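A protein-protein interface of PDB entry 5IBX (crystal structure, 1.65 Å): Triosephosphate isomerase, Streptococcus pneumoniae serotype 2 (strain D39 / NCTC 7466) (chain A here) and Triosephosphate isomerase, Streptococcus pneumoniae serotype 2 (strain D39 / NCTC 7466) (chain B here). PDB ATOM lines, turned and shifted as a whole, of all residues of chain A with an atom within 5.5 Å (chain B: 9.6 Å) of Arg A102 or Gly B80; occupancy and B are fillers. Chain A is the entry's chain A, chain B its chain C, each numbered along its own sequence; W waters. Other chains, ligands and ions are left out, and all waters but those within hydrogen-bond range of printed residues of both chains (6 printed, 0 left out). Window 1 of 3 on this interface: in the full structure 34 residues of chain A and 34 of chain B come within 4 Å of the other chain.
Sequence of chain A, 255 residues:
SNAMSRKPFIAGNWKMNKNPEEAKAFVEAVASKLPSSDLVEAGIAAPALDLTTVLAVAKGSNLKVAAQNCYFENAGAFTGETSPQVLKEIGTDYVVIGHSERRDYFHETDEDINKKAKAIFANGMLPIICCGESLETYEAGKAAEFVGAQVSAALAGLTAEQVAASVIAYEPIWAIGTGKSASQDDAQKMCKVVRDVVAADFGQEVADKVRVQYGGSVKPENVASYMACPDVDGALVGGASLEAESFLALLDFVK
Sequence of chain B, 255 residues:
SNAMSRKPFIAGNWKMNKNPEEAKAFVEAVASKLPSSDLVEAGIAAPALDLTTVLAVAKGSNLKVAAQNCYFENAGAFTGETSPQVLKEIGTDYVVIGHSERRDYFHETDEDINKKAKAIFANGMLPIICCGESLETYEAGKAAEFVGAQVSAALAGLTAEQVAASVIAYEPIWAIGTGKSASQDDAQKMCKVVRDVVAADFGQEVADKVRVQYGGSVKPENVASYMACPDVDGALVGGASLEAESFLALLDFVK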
ATOM      1  N   LYS A  15     -29.926   3.709 -34.257  1.00  0.00           N
ATOM      2  CA  LYS A  15     -30.265   3.320 -32.877  1.00  0.00           C
ATOM      3  C   LYS A  15     -29.735   1.911 -32.559  1.00  0.00           C
ATOM      4  O   LYS A  15     -28.690   1.550 -33.077  1.00  0.00           O
ATOM      5  CB  LYS A  15     -31.750   3.508 -32.573  1.00  0.00           C
ATOM      6  CG  LYS A  15     -32.222   4.916 -32.907  1.00  0.00           C
ATOM      7  CD  LYS A  15     -33.698   5.062 -32.582  1.00  0.00           C
ATOM      8  CE  LYS A  15     -34.243   6.458 -32.897  1.00  0.00           C
ATOM      9  NZ  LYS A  15     -35.663   6.600 -32.485  1.00  0.00           N
ATOM     10  N   MET A  16     -30.390   1.124 -31.698  1.00  0.00           N
ATOM     11  CA  MET A  16     -29.838  -0.174 -31.336  1.00  0.00           C
ATOM     12  C   MET A  16     -30.287  -1.263 -32.328  1.00  0.00           C
ATOM     13  O   MET A  16     -31.153  -2.083 -32.008  1.00  0.00           O
ATOM     14  CB  MET A  16     -30.192  -0.534 -29.906  1.00  0.00           C
ATOM     15  CG  MET A  16     -29.386  -1.714 -29.424  1.00  0.00           C
ATOM     16  SD  MET A  16     -29.672  -2.244 -27.756  1.00  0.00           S
ATOM     17  CE  MET A  16     -31.330  -2.910 -27.813  1.00  0.00           C
ATOM     18  N   GLN A  68     -23.194   6.923 -31.467  1.00  0.00           N
ATOM     19  CA  GLN A  68     -24.511   7.284 -30.896  1.00  0.00           C
ATOM     20  C   GLN A  68     -24.447   7.869 -29.495  1.00  0.00           C
ATOM     21  O   GLN A  68     -25.478   8.246 -28.936  1.00  0.00           O
ATOM     22  CB  GLN A  68     -25.447   6.083 -30.861  1.00  0.00           C
ATOM     23  CG  GLN A  68     -25.926   5.672 -32.234  1.00  0.00           C
ATOM     24  CD  GLN A  68     -26.674   4.347 -32.272  1.00  0.00           C
ATOM     25  OE1 GLN A  68     -27.133   3.809 -31.249  1.00  0.00           O
ATOM     26  NE2 GLN A  68     -26.781   3.804 -33.452  1.00  0.00           N
ATOM     27  N   ASN A  69     -23.246   7.880 -28.913  1.00  0.00           N
ATOM     28  CA  ASN A  69     -23.012   8.358 -27.557  1.00  0.00           C
ATOM     29  C   ASN A  69     -21.530   8.137 -27.241  1.00  0.00           C
ATOM     30  O   ASN A  69     -20.874   7.302 -27.881  1.00  0.00           O
ATOM     31  CB  ASN A  69     -23.796   7.520 -26.528  1.00  0.00           C
ATOM     32  CG  ASN A  69     -23.604   8.014 -25.118  1.00  0.00           C
ATOM     33  OD1 ASN A  69     -23.553   9.226 -24.864  1.00  0.00           O
ATOM     34  ND2 ASN A  69     -23.456   7.064 -24.168  1.00  0.00           N
ATOM     35  N   GLY A  98     -27.014  13.476 -26.143  1.00  0.00           N
ATOM     36  CA  GLY A  98     -28.222  14.045 -25.618  1.00  0.00           C
ATOM     37  C   GLY A  98     -29.486  13.621 -26.315  1.00  0.00           C
ATOM     38  O   GLY A  98     -30.526  14.265 -26.155  1.00  0.00           O
ATOM     39  N   HIS A  99     -29.428  12.497 -27.027  1.00  0.00           N
ATOM     40  CA  HIS A  99     -30.603  11.991 -27.691  1.00  0.00           C
ATOM     41  C   HIS A  99     -31.708  11.785 -26.658  1.00  0.00           C
ATOM     42  O   HIS A  99     -31.438  11.345 -25.497  1.00  0.00           O
ATOM     43  CB  HIS A  99     -30.291  10.677 -28.380  1.00  0.00           C
ATOM     44  CG  HIS A  99     -31.343  10.261 -29.325  1.00  0.00           C
ATOM     45  ND1 HIS A  99     -32.465   9.578 -28.928  1.00  0.00           N
ATOM     46  CD2 HIS A  99     -31.501  10.513 -30.642  1.00  0.00           C
ATOM     47  CE1 HIS A  99     -33.245   9.370 -29.964  1.00  0.00           C
ATOM     48  NE2 HIS A  99     -32.706   9.958 -31.010  1.00  0.00           N
ATOM     49  N   SER A 100     -32.947  12.089 -27.034  1.00  0.00           N
ATOM     50  CA  SER A 100     -34.078  11.928 -26.145  1.00  0.00           C
ATOM     51  C   SER A 100     -34.104  10.579 -25.391  1.00  0.00           C
ATOM     52  O   SER A 100     -34.498  10.490 -24.214  1.00  0.00           O
ATOM     53  CB  SER A 100     -35.412  12.128 -26.901  1.00  0.00           C
ATOM     54  OG  SER A 100     -35.598  11.176 -27.960  1.00  0.00           O
ATOM     55  N   GLU A 101     -33.757   9.510 -26.083  1.00  0.00           N
ATOM     56  CA  GLU A 101     -33.788   8.190 -25.462  1.00  0.00           C
ATOM     57  C   GLU A 101     -32.782   8.063 -24.341  1.00  0.00           C
ATOM     58  O   GLU A 101     -33.046   7.376 -23.342  1.00  0.00           O
ATOM     59  CB  GLU A 101     -33.602   7.089 -26.527  1.00  0.00           C
ATOM     60  CG  GLU A 101     -34.833   6.900 -27.402  1.00  0.00           C
ATOM     61  CD  GLU A 101     -34.507   6.476 -28.834  1.00  0.00           C
ATOM     62  OE1 GLU A 101     -33.412   5.951 -29.139  1.00  0.00           O
ATOM     63  OE2 GLU A 101     -35.396   6.675 -29.684  1.00  0.00           O
ATOM     64  N   ARG A 102     -31.652   8.751 -24.473  1.00  0.00           N
ATOM     65  CA  ARG A 102     -30.627   8.678 -23.427  1.00  0.00           C
ATOM     66  C   ARG A 102     -30.971   9.610 -22.235  1.00  0.00           C
ATOM     67  O   ARG A 102     -30.689   9.279 -21.077  1.00  0.00           O
ATOM     68  CB  ARG A 102     -29.263   8.920 -23.997  1.00  0.00           C
ATOM     69  CG  ARG A 102     -28.887   7.890 -25.072  1.00  0.00           C
ATOM     70  CD  ARG A 102     -27.388   7.714 -25.177  1.00  0.00           C
ATOM     71  NE  ARG A 102     -26.853   7.196 -23.918  1.00  0.00           N
ATOM     72  CZ  ARG A 102     -26.876   5.906 -23.563  1.00  0.00           C
ATOM     73  NH1 ARG A 102     -27.388   4.989 -24.368  1.00  0.00           N
ATOM     74  NH2 ARG A 102     -26.360   5.521 -22.409  1.00  0.00           N
ATOM     75  N   ARG A 103     -31.565  10.766 -22.524  1.00  0.00           N
ATOM     76  CA  ARG A 103     -31.982  11.670 -21.467  1.00  0.00           C
ATOM     77  C   ARG A 103     -33.121  10.996 -20.700  1.00  0.00           C
ATOM     78  O   ARG A 103     -33.266  11.215 -19.489  1.00  0.00           O
ATOM     79  CB  ARG A 103     -32.453  13.015 -22.012  1.00  0.00           C
ATOM     80  CG  ARG A 103     -31.369  13.850 -22.659  1.00  0.00           C
ATOM     81  CD  ARG A 103     -31.999  15.085 -23.280  1.00  0.00           C
ATOM     82  NE  ARG A 103     -31.124  15.964 -24.038  1.00  0.00           N
ATOM     83  CZ  ARG A 103     -30.482  17.043 -23.569  1.00  0.00           C
ATOM     84  NH1 ARG A 103     -30.534  17.347 -22.277  1.00  0.00           N
ATOM     85  NH2 ARG A 103     -29.760  17.837 -24.414  1.00  0.00           N
ATOM     86  N   ASP A 104     -33.876  10.139 -21.401  1.00  0.00           N
ATOM     87  CA  ASP A 104     -34.981   9.397 -20.787  1.00  0.00           C
ATOM     88  C   ASP A 104     -34.477   8.154 -20.038  1.00  0.00           C
ATOM     89  O   ASP A 104     -34.275   8.189 -18.824  1.00  0.00           O
ATOM     90  CB  ASP A 104     -36.044   9.064 -21.857  1.00  0.00           C
ATOM     91  CG  ASP A 104     -37.204   8.220 -21.343  1.00  0.00           C
ATOM     92  OD1 ASP A 104     -37.370   8.049 -20.124  1.00  0.00           O
ATOM     93  OD2 ASP A 104     -37.940   7.672 -22.212  1.00  0.00           O
ATOM     94  N   TYR A 105     -34.217   7.071 -20.750  1.00  0.00           N
ATOM     95  CA  TYR A 105     -33.884   5.825 -20.089  1.00  0.00           C
ATOM     96  C   TYR A 105     -32.633   5.848 -19.245  1.00  0.00           C
ATOM     97  O   TYR A 105     -32.604   5.195 -18.193  1.00  0.00           O
ATOM     98  CB  TYR A 105     -33.737   4.675 -21.098  1.00  0.00           C
ATOM     99  CG  TYR A 105     -34.955   4.435 -21.987  1.00  0.00           C
ATOM    100  CD1 TYR A 105     -36.114   3.913 -21.469  1.00  0.00           C
ATOM    101  CD2 TYR A 105     -34.894   4.672 -23.360  1.00  0.00           C
ATOM    102  CE1 TYR A 105     -37.215   3.666 -22.273  1.00  0.00           C
ATOM    103  CE2 TYR A 105     -35.997   4.437 -24.175  1.00  0.00           C
ATOM    104  CZ  TYR A 105     -37.157   3.957 -23.606  1.00  0.00           C
ATOM    105  OH  TYR A 105     -38.271   3.691 -24.389  1.00  0.00           O
ATOM    106  N   PHE A 106     -31.604   6.544 -19.738  1.00  0.00           N
ATOM    107  CA  PHE A 106     -30.255   6.510 -19.167  1.00  0.00           C
ATOM    108  C   PHE A 106     -29.841   7.762 -18.378  1.00  0.00           C
ATOM    109  O   PHE A 106     -28.638   7.997 -18.097  1.00  0.00           O
ATOM    110  CB  PHE A 106     -29.292   6.077 -20.269  1.00  0.00           C
ATOM    111  CG  PHE A 106     -29.792   4.846 -21.005  1.00  0.00           C
ATOM    112  CD1 PHE A 106     -30.005   3.665 -20.297  1.00  0.00           C
ATOM    113  CD2 PHE A 106     -30.162   4.874 -22.360  1.00  0.00           C
ATOM    114  CE1 PHE A 106     -30.547   2.551 -20.914  1.00  0.00           C
ATOM    115  CE2 PHE A 106     -30.711   3.738 -22.975  1.00  0.00           C
ATOM    116  CZ  PHE A 106     -30.898   2.576 -22.251  1.00  0.00           C
ATOM    117  N   HIS A 107     -30.849   8.531 -17.992  1.00  0.00           N
ATOM    118  CA  HIS A 107     -30.679   9.647 -17.043  1.00  0.00           C
ATOM    119  C   HIS A 107     -29.697  10.757 -17.454  1.00  0.00           C
ATOM    120  O   HIS A 107     -29.219  11.487 -16.609  1.00  0.00           O
ATOM    121  CB  HIS A 107     -30.236   9.079 -15.647  1.00  0.00           C
ATOM    122  CG  HIS A 107     -30.963   7.834 -15.237  1.00  0.00           C
ATOM    123  ND1 HIS A 107     -32.266   7.836 -14.786  1.00  0.00           N
ATOM    124  CD2 HIS A 107     -30.559   6.541 -15.206  1.00  0.00           C
ATOM    125  CE1 HIS A 107     -32.626   6.602 -14.484  1.00  0.00           C
ATOM    126  NE2 HIS A 107     -31.614   5.795 -14.744  1.00  0.00           N
ATOM    127  N   GLU A 108     -29.421  10.922 -18.733  1.00  0.00           N
ATOM    128  CA  GLU A 108     -28.429  11.949 -19.127  1.00  0.00           C
ATOM    129  C   GLU A 108     -28.957  13.331 -18.860  1.00  0.00           C
ATOM    130  O   GLU A 108     -30.127  13.632 -19.146  1.00  0.00           O
ATOM    131  CB  GLU A 108     -28.025  11.800 -20.586  1.00  0.00           C
ATOM    132  CG  GLU A 108     -27.412  10.446 -20.845  1.00  0.00           C
ATOM    133  CD  GLU A 108     -26.608  10.392 -22.117  1.00  0.00           C
ATOM    134  OE1 GLU A 108     -26.787  11.307 -22.953  1.00  0.00           O
ATOM    135  OE2 GLU A 108     -25.823   9.410 -22.270  1.00  0.00           O
ATOM    136  N   LYS A 116     -19.741  16.155 -22.496  1.00  0.00           N
ATOM    137  CA  LYS A 116     -19.536  15.347 -23.682  1.00  0.00           C
ATOM    138  C   LYS A 116     -19.133  16.208 -24.887  1.00  0.00           C
ATOM    139  O   LYS A 116     -18.223  15.858 -25.611  1.00  0.00           O
ATOM    140  CB  LYS A 116     -20.775  14.504 -23.978  1.00  0.00           C
ATOM    141  CG  LYS A 116     -20.940  13.351 -22.991  1.00  0.00           C
ATOM    142  CD  LYS A 116     -22.196  12.518 -23.198  1.00  0.00           C
ATOM    143  CE  LYS A 116     -22.240  11.460 -22.090  1.00  0.00           C
ATOM    144  NZ  LYS A 116     -23.240  10.408 -22.262  1.00  0.00           N
ATOM    145  N   ALA B  48     -16.887  -2.085 -26.028  1.00  0.00           N
ATOM    146  CA  ALA B  48     -17.644  -2.484 -27.204  1.00  0.00           C
ATOM    147  C   ALA B  48     -16.948  -2.160 -28.510  1.00  0.00           C
ATOM    148  O   ALA B  48     -17.054  -2.971 -29.455  1.00  0.00           O
ATOM    149  CB  ALA B  48     -19.040  -1.876 -27.204  1.00  0.00           C
ATOM    150  N   ASN B  69     -21.069  -4.569 -20.495  1.00  0.00           N
ATOM    151  CA  ASN B  69     -22.442  -4.215 -20.249  1.00  0.00           C
ATOM    152  C   ASN B  69     -23.249  -4.496 -21.516  1.00  0.00           C
ATOM    153  O   ASN B  69     -22.672  -4.642 -22.590  1.00  0.00           O
ATOM    154  CB  ASN B  69     -22.575  -2.707 -19.930  1.00  0.00           C
ATOM    155  CG  ASN B  69     -24.010  -2.292 -19.684  1.00  0.00           C
ATOM    156  OD1 ASN B  69     -24.706  -2.866 -18.844  1.00  0.00           O
ATOM    157  ND2 ASN B  69     -24.436  -1.276 -20.384  1.00  0.00           N
ATOM    158  N   CYS B  70     -24.578  -4.554 -21.375  1.00  0.00           N
ATOM    159  CA  CYS B  70     -25.482  -4.652 -22.519  1.00  0.00           C
ATOM    160  C   CYS B  70     -26.864  -4.208 -22.028  1.00  0.00           C
ATOM    161  O   CYS B  70     -27.085  -4.064 -20.839  1.00  0.00           O
ATOM    162  CB  CYS B  70     -25.538  -6.081 -23.081  1.00  0.00           C
ATOM    163  SG  CYS B  70     -26.351  -7.289 -21.999  1.00  0.00           S
ATOM    164  N   TYR B  71     -27.774  -3.956 -22.955  1.00  0.00           N
ATOM    165  CA  TYR B  71     -29.134  -3.596 -22.619  1.00  0.00           C
ATOM    166  C   TYR B  71     -29.963  -4.865 -22.505  1.00  0.00           C
ATOM    167  O   TYR B  71     -29.455  -5.960 -22.734  1.00  0.00           O
ATOM    168  CB  TYR B  71     -29.718  -2.643 -23.671  1.00  0.00           C
ATOM    169  CG  TYR B  71     -31.005  -1.943 -23.216  1.00  0.00           C
ATOM    170  CD1 TYR B  71     -31.057  -1.248 -22.011  1.00  0.00           C
ATOM    171  CD2 TYR B  71     -32.132  -1.956 -23.991  1.00  0.00           C
ATOM    172  CE1 TYR B  71     -32.207  -0.602 -21.611  1.00  0.00           C
ATOM    173  CE2 TYR B  71     -33.282  -1.316 -23.615  1.00  0.00           C
ATOM    174  CZ  TYR B  71     -33.321  -0.625 -22.422  1.00  0.00           C
ATOM    175  OH  TYR B  71     -34.490   0.010 -22.037  1.00  0.00           O
ATOM    176  N   GLY B  76     -33.910  -2.087 -30.995  1.00  0.00           N
ATOM    177  CA  GLY B  76     -34.945  -1.063 -30.922  1.00  0.00           C
ATOM    178  C   GLY B  76     -34.446   0.334 -30.704  1.00  0.00           C
ATOM    179  O   GLY B  76     -33.260   0.620 -30.873  1.00  0.00           O
ATOM    180  N   ALA B  77     -35.374   1.153 -30.230  1.00  0.00           N
ATOM    181  CA  ALA B  77     -35.176   2.607 -30.104  1.00  0.00           C
ATOM    182  C   ALA B  77     -34.479   2.962 -28.802  1.00  0.00           C
ATOM    183  O   ALA B  77     -35.033   3.631 -27.915  1.00  0.00           O
ATOM    184  CB  ALA B  77     -36.511   3.317 -30.271  1.00  0.00           C
ATOM    185  N   PHE B  78     -33.230   2.522 -28.733  1.00  0.00           N
ATOM    186  CA  PHE B  78     -32.377   2.693 -27.550  1.00  0.00           C
ATOM    187  C   PHE B  78     -31.006   3.206 -27.982  1.00  0.00           C
ATOM    188  O   PHE B  78     -29.987   2.508 -27.885  1.00  0.00           O
ATOM    189  CB  PHE B  78     -32.287   1.379 -26.780  1.00  0.00           C
ATOM    190  CG  PHE B  78     -33.611   0.797 -26.492  1.00  0.00           C
ATOM    191  CD1 PHE B  78     -34.425   1.362 -25.547  1.00  0.00           C
ATOM    192  CD2 PHE B  78     -34.082  -0.273 -27.218  1.00  0.00           C
ATOM    193  CE1 PHE B  78     -35.694   0.866 -25.311  1.00  0.00           C
ATOM    194  CE2 PHE B  78     -35.355  -0.791 -26.988  1.00  0.00           C
ATOM    195  CZ  PHE B  78     -36.154  -0.222 -26.022  1.00  0.00           C
ATOM    196  N   THR B  79     -31.001   4.464 -28.413  1.00  0.00           N
ATOM    197  CA  THR B  79     -29.800   5.087 -28.943  1.00  0.00           C
ATOM    198  C   THR B  79     -28.625   4.975 -27.975  1.00  0.00           C
ATOM    199  O   THR B  79     -28.752   5.303 -26.801  1.00  0.00           O
ATOM    200  CB  THR B  79     -30.099   6.559 -29.295  1.00  0.00           C
ATOM    201  OG1 THR B  79     -31.086   6.589 -30.342  1.00  0.00           O
ATOM    202  CG2 THR B  79     -28.871   7.278 -29.739  1.00  0.00           C
ATOM    203  N   GLY B  80     -27.511   4.477 -28.479  1.00  0.00           N
ATOM    204  CA  GLY B  80     -26.286   4.360 -27.702  1.00  0.00           C
ATOM    205  C   GLY B  80     -26.085   3.070 -26.947  1.00  0.00           C
ATOM    206  O   GLY B  80     -24.989   2.847 -26.383  1.00  0.00           O
ATOM    207  N   GLU B  81     -27.080   2.182 -26.971  1.00  0.00           N
ATOM    208  CA  GLU B  81     -27.005   0.880 -26.272  1.00  0.00           C
ATOM    209  C   GLU B  81     -26.406  -0.291 -27.068  1.00  0.00           C
ATOM    210  O   GLU B  81     -26.461  -0.341 -28.314  1.00  0.00           O
ATOM    211  CB  GLU B  81     -28.399   0.478 -25.729  1.00  0.00           C
ATOM    212  CG  GLU B  81     -28.872   1.409 -24.620  1.00  0.00           C
ATOM    213  CD  GLU B  81     -27.915   1.417 -23.462  1.00  0.00           C
ATOM    214  OE1 GLU B  81     -27.817   0.348 -22.763  1.00  0.00           O
ATOM    215  OE2 GLU B  81     -27.301   2.486 -23.210  1.00  0.00           O
ATOM    216  N   THR B  82     -25.824  -1.216 -26.321  1.00  0.00           N
ATOM    217  CA  THR B  82     -25.208  -2.410 -26.873  1.00  0.00           C
ATOM    218  C   THR B  82     -26.180  -3.579 -26.760  1.00  0.00           C
ATOM    219  O   THR B  82     -26.655  -3.900 -25.685  1.00  0.00           O
ATOM    220  CB  THR B  82     -23.853  -2.679 -26.174  1.00  0.00           C
ATOM    221  OG1 THR B  82     -22.940  -1.662 -26.591  1.00  0.00           O
ATOM    222  CG2 THR B  82     -23.284  -4.028 -26.557  1.00  0.00           C
ATOM    223  N   SER B  83     -26.459  -4.217 -27.890  1.00  0.00           N
ATOM    224  CA  SER B  83     -27.417  -5.335 -27.948  1.00  0.00           C
ATOM    225  C   SER B  83     -26.810  -6.689 -27.565  1.00  0.00           C
ATOM    226  O   SER B  83     -25.736  -7.019 -28.050  1.00  0.00           O
ATOM    227  CB  SER B  83     -27.970  -5.457 -29.347  1.00  0.00           C
ATOM    228  OG  SER B  83     -28.630  -6.703 -29.521  1.00  0.00           O
ATOM    229  N   ARG B 102     -21.416   1.211 -12.919  1.00  0.00           N
ATOM    230  CA  ARG B 102     -22.681   1.432 -13.632  1.00  0.00           C
ATOM    231  C   ARG B 102     -23.828   1.663 -12.660  1.00  0.00           C
ATOM    232  O   ARG B 102     -24.728   2.419 -12.922  1.00  0.00           O
ATOM    233  CB  ARG B 102     -22.978   0.298 -14.603  1.00  0.00           C
ATOM    234  CG  ARG B 102     -21.902   0.146 -15.650  1.00  0.00           C
ATOM    235  CD  ARG B 102     -22.400  -0.409 -16.937  1.00  0.00           C
ATOM    236  NE  ARG B 102     -23.329   0.508 -17.547  1.00  0.00           N
ATOM    237  CZ  ARG B 102     -23.004   1.568 -18.289  1.00  0.00           C
ATOM    238  NH1 ARG B 102     -21.729   1.840 -18.566  1.00  0.00           N
ATOM    239  NH2 ARG B 102     -23.965   2.340 -18.794  1.00  0.00           N
ATOM    240  N   TYR B 105     -22.566   5.675 -11.501  1.00  0.00           N
ATOM    241  CA  TYR B 105     -22.699   6.759 -12.474  1.00  0.00           C
ATOM    242  C   TYR B 105     -23.991   6.739 -13.285  1.00  0.00           C
ATOM    243  O   TYR B 105     -24.522   7.798 -13.623  1.00  0.00           O
ATOM    244  CB  TYR B 105     -21.526   6.766 -13.454  1.00  0.00           C
ATOM    245  CG  TYR B 105     -20.163   6.977 -12.819  1.00  0.00           C
ATOM    246  CD1 TYR B 105     -19.848   8.162 -12.185  1.00  0.00           C
ATOM    247  CD2 TYR B 105     -19.194   5.993 -12.888  1.00  0.00           C
ATOM    248  CE1 TYR B 105     -18.595   8.366 -11.620  1.00  0.00           C
ATOM    249  CE2 TYR B 105     -17.952   6.167 -12.316  1.00  0.00           C
ATOM    250  CZ  TYR B 105     -17.668   7.354 -11.655  1.00  0.00           C
ATOM    251  OH  TYR B 105     -16.445   7.557 -11.086  1.00  0.00           O
ATOM    252  N   PHE B 106     -24.476   5.553 -13.593  1.00  0.00           N
ATOM    253  CA  PHE B 106     -25.645   5.413 -14.461  1.00  0.00           C
ATOM    254  C   PHE B 106     -26.905   4.933 -13.756  1.00  0.00           C
ATOM    255  O   PHE B 106     -27.926   4.631 -14.399  1.00  0.00           O
ATOM    256  CB  PHE B 106     -25.223   4.539 -15.621  1.00  0.00           C
ATOM    257  CG  PHE B 106     -24.003   5.066 -16.300  1.00  0.00           C
ATOM    258  CD1 PHE B 106     -24.069   6.285 -16.958  1.00  0.00           C
ATOM    259  CD2 PHE B 106     -22.768   4.442 -16.178  1.00  0.00           C
ATOM    260  CE1 PHE B 106     -22.939   6.843 -17.533  1.00  0.00           C
ATOM    261  CE2 PHE B 106     -21.636   4.997 -16.736  1.00  0.00           C
ATOM    262  CZ  PHE B 106     -21.724   6.200 -17.427  1.00  0.00           C
ATOM    263  N   HIS B 107     -26.870   4.928 -12.425  1.00  0.00           N
ATOM    264  CA  HIS B 107     -28.058   4.605 -11.614  1.00  0.00           C
ATOM    265  C   HIS B 107     -28.725   3.272 -11.964  1.00  0.00           C
ATOM    266  O   HIS B 107     -29.929   3.133 -11.837  1.00  0.00           O
ATOM    267  CB  HIS B 107     -29.093   5.749 -11.722  1.00  0.00           C
ATOM    268  CG  HIS B 107     -28.509   7.125 -11.561  1.00  0.00           C
ATOM    269  ND1 HIS B 107     -27.832   7.520 -10.422  1.00  0.00           N
ATOM    270  CD2 HIS B 107     -28.526   8.206 -12.379  1.00  0.00           C
ATOM    271  CE1 HIS B 107     -27.451   8.778 -10.553  1.00  0.00           C
ATOM    272  NE2 HIS B 107     -27.861   9.220 -11.734  1.00  0.00           N
ATOM    273  N   GLU B 108     -27.944   2.273 -12.360  1.00  0.00           N
ATOM    274  CA  GLU B 108     -28.555   1.001 -12.758  1.00  0.00           C
ATOM    275  C   GLU B 108     -29.138   0.338 -11.534  1.00  0.00           C
ATOM    276  O   GLU B 108     -28.501   0.347 -10.477  1.00  0.00           O
ATOM    277  CB  GLU B 108     -27.567   0.081 -13.455  1.00  0.00           C
ATOM    278  CG  GLU B 108     -27.033   0.655 -14.781  1.00  0.00           C
ATOM    279  CD  GLU B 108     -26.381  -0.379 -15.680  1.00  0.00           C
ATOM    280  OE1 GLU B 108     -26.181  -1.519 -15.226  1.00  0.00           O
ATOM    281  OE2 GLU B 108     -26.053  -0.039 -16.850  1.00  0.00           O
ATOM    282  N   LYS B 116     -31.304  -7.850 -17.444  1.00  0.00           N
ATOM    283  CA  LYS B 116     -30.115  -8.108 -18.239  1.00  0.00           C
ATOM    284  C   LYS B 116     -29.695  -9.594 -18.126  1.00  0.00           C
ATOM    285  O   LYS B 116     -29.387 -10.227 -19.099  1.00  0.00           O
ATOM    286  CB  LYS B 116     -28.982  -7.197 -17.832  1.00  0.00           C
ATOM    287  CG  LYS B 116     -29.179  -5.767 -18.334  1.00  0.00           C
ATOM    288  CD  LYS B 116     -28.096  -4.818 -17.911  1.00  0.00           C
ATOM    289  CE  LYS B 116     -28.524  -3.414 -18.310  1.00  0.00           C
ATOM    290  NZ  LYS B 116     -27.433  -2.432 -18.256  1.00  0.00           N
HETATM  291  O   HOH W   1     -23.055   4.303 -24.696  1.00  0.00           O
HETATM  292  O   HOH W   2     -37.675   3.589 -27.018  1.00  0.00           O
HETATM  293  O   HOH W   3     -26.014   1.518 -30.141  1.00  0.00           O
HETATM  294  O   HOH W   4     -31.980   2.983 -13.928  1.00  0.00           O
HETATM  295  O   HOH W   5     -26.045   2.887 -20.919  1.00  0.00           O
HETATM  296  O   HOH W   6     -24.069   4.871 -20.345  1.00  0.00           O
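The side-chain amide oxygen (OE1) of Gln A68 sits at hydrogen-bond distance from the backbone NH (N) of Gly B80 (2.9 Å).
SD of Met A16 sits close to O of Glu B81, at 3.8 Å.
The backbone NH (N) of Phe B78 sits at hydrogen-bond distance from the side-chain carboxylate (OE1) of Glu A101 (3.5 Å).
The guanidinium group (NH1) of Arg A102 lies within salt-bridge range of the side-chain carboxylate (OE2) of Glu B81, at 2.8 Å.
The backbone carbonyl oxygen (O) of Met A16 is in hydrogen-bond range of the backbone NH (N) of Gly B76, 2.9 Å away.
OE1 of Glu A101 lies within hydrogen-bond range of OG1 of Thr B79 (2.7 Å).
The guanidinium group of Arg A102 is in hydrogen-bond range of the backbone carbonyl oxygen of Thr B79 (2.8 Å).
OE1 of Glu A101 sits close to O of Ala B77, at 3.1 Å.
SD of Met A16 lies within hydrogen-bond range of N of Ser B83, at 3.8 Å.
The side-chain amino group (NZ) of Lys A15 is in salt-bridge range of the side-chain carboxylate (OE2) of Glu A101, at 2.8 Å.
The backbone NH of His B107 is in hydrogen-bond range of the backbone carbonyl oxygen of Arg B102.
ND1 of His A99 sits close to N of Glu A101 (3.1 Å).
Phe B78 touches Met A16.
O of Gln A68 touches CG2 of Thr B79 (3.6 Å).
CE1 of His A99 touches OG1 of Thr B79, at 3.5 Å.
C of Gly B80 touches NH1 of Arg A102, 3.5 Å away.
His A107 touches Phe B106.
CG of His A107 touches CD2 of His B107, 3.8 Å away.
Gln A68 touches just these residues of chain B: Thr B79 (3.6 Å) and Gly B80 (2.9 Å).
Of chain B, only Thr B79, Gly B80 and Glu B81 come within 4 Å of Arg A102.
Asp A104 touches none of the printed residues of chain B.
Of chain B, only Tyr B71 and Glu B81 come within 4 Å of Phe A106.
No residue of chain B comes within 4 Å of Glu A108.
Tyr B105 touches none of the printed residues of chain A.
Of the printed residues of chain A, Phe B106 touches His A107 (3.4 Å).
The nearest residue of chain A that does not touch Gly B80 is Asn A69 (4.2 Å).
Of the 18 printed residues of chain B, 11 touch a printed residue of chain A.
Hydrophobic or aromatic side chains of chain B that line the printed part of chain A: Tyr B71, Ala B77, Phe B78 and His B107.
Printed residues of chain A that touch a printed residue of chain B: Lys A15, Met A16, Gln A68, His A99, Glu A101, Arg A102, Tyr A105, Phe A106 and His A107.
Hydrophobic or aromatic side chains of chain A within 4 Å of the printed part of chain B: Met A16, His A99, Tyr A105, Phe A106 and His A107.
Among the printed residues, Asp or Glu carboxylates within 4 Å of a Lys or Arg side-chain nitrogen of the other chain: Arg A102 with Glu B81 (2.8 Å).
Water W2 bridges the side-chain hydroxyl (OH) of Tyr A105 and the backbone carbonyl oxygen (O) of Ala B77.
Water W1 bridges the side-chain amide nitrogen of Asn A69 (2.8 Å) and the backbone carbonyl oxygen of Gly B80 (3.0 Å).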
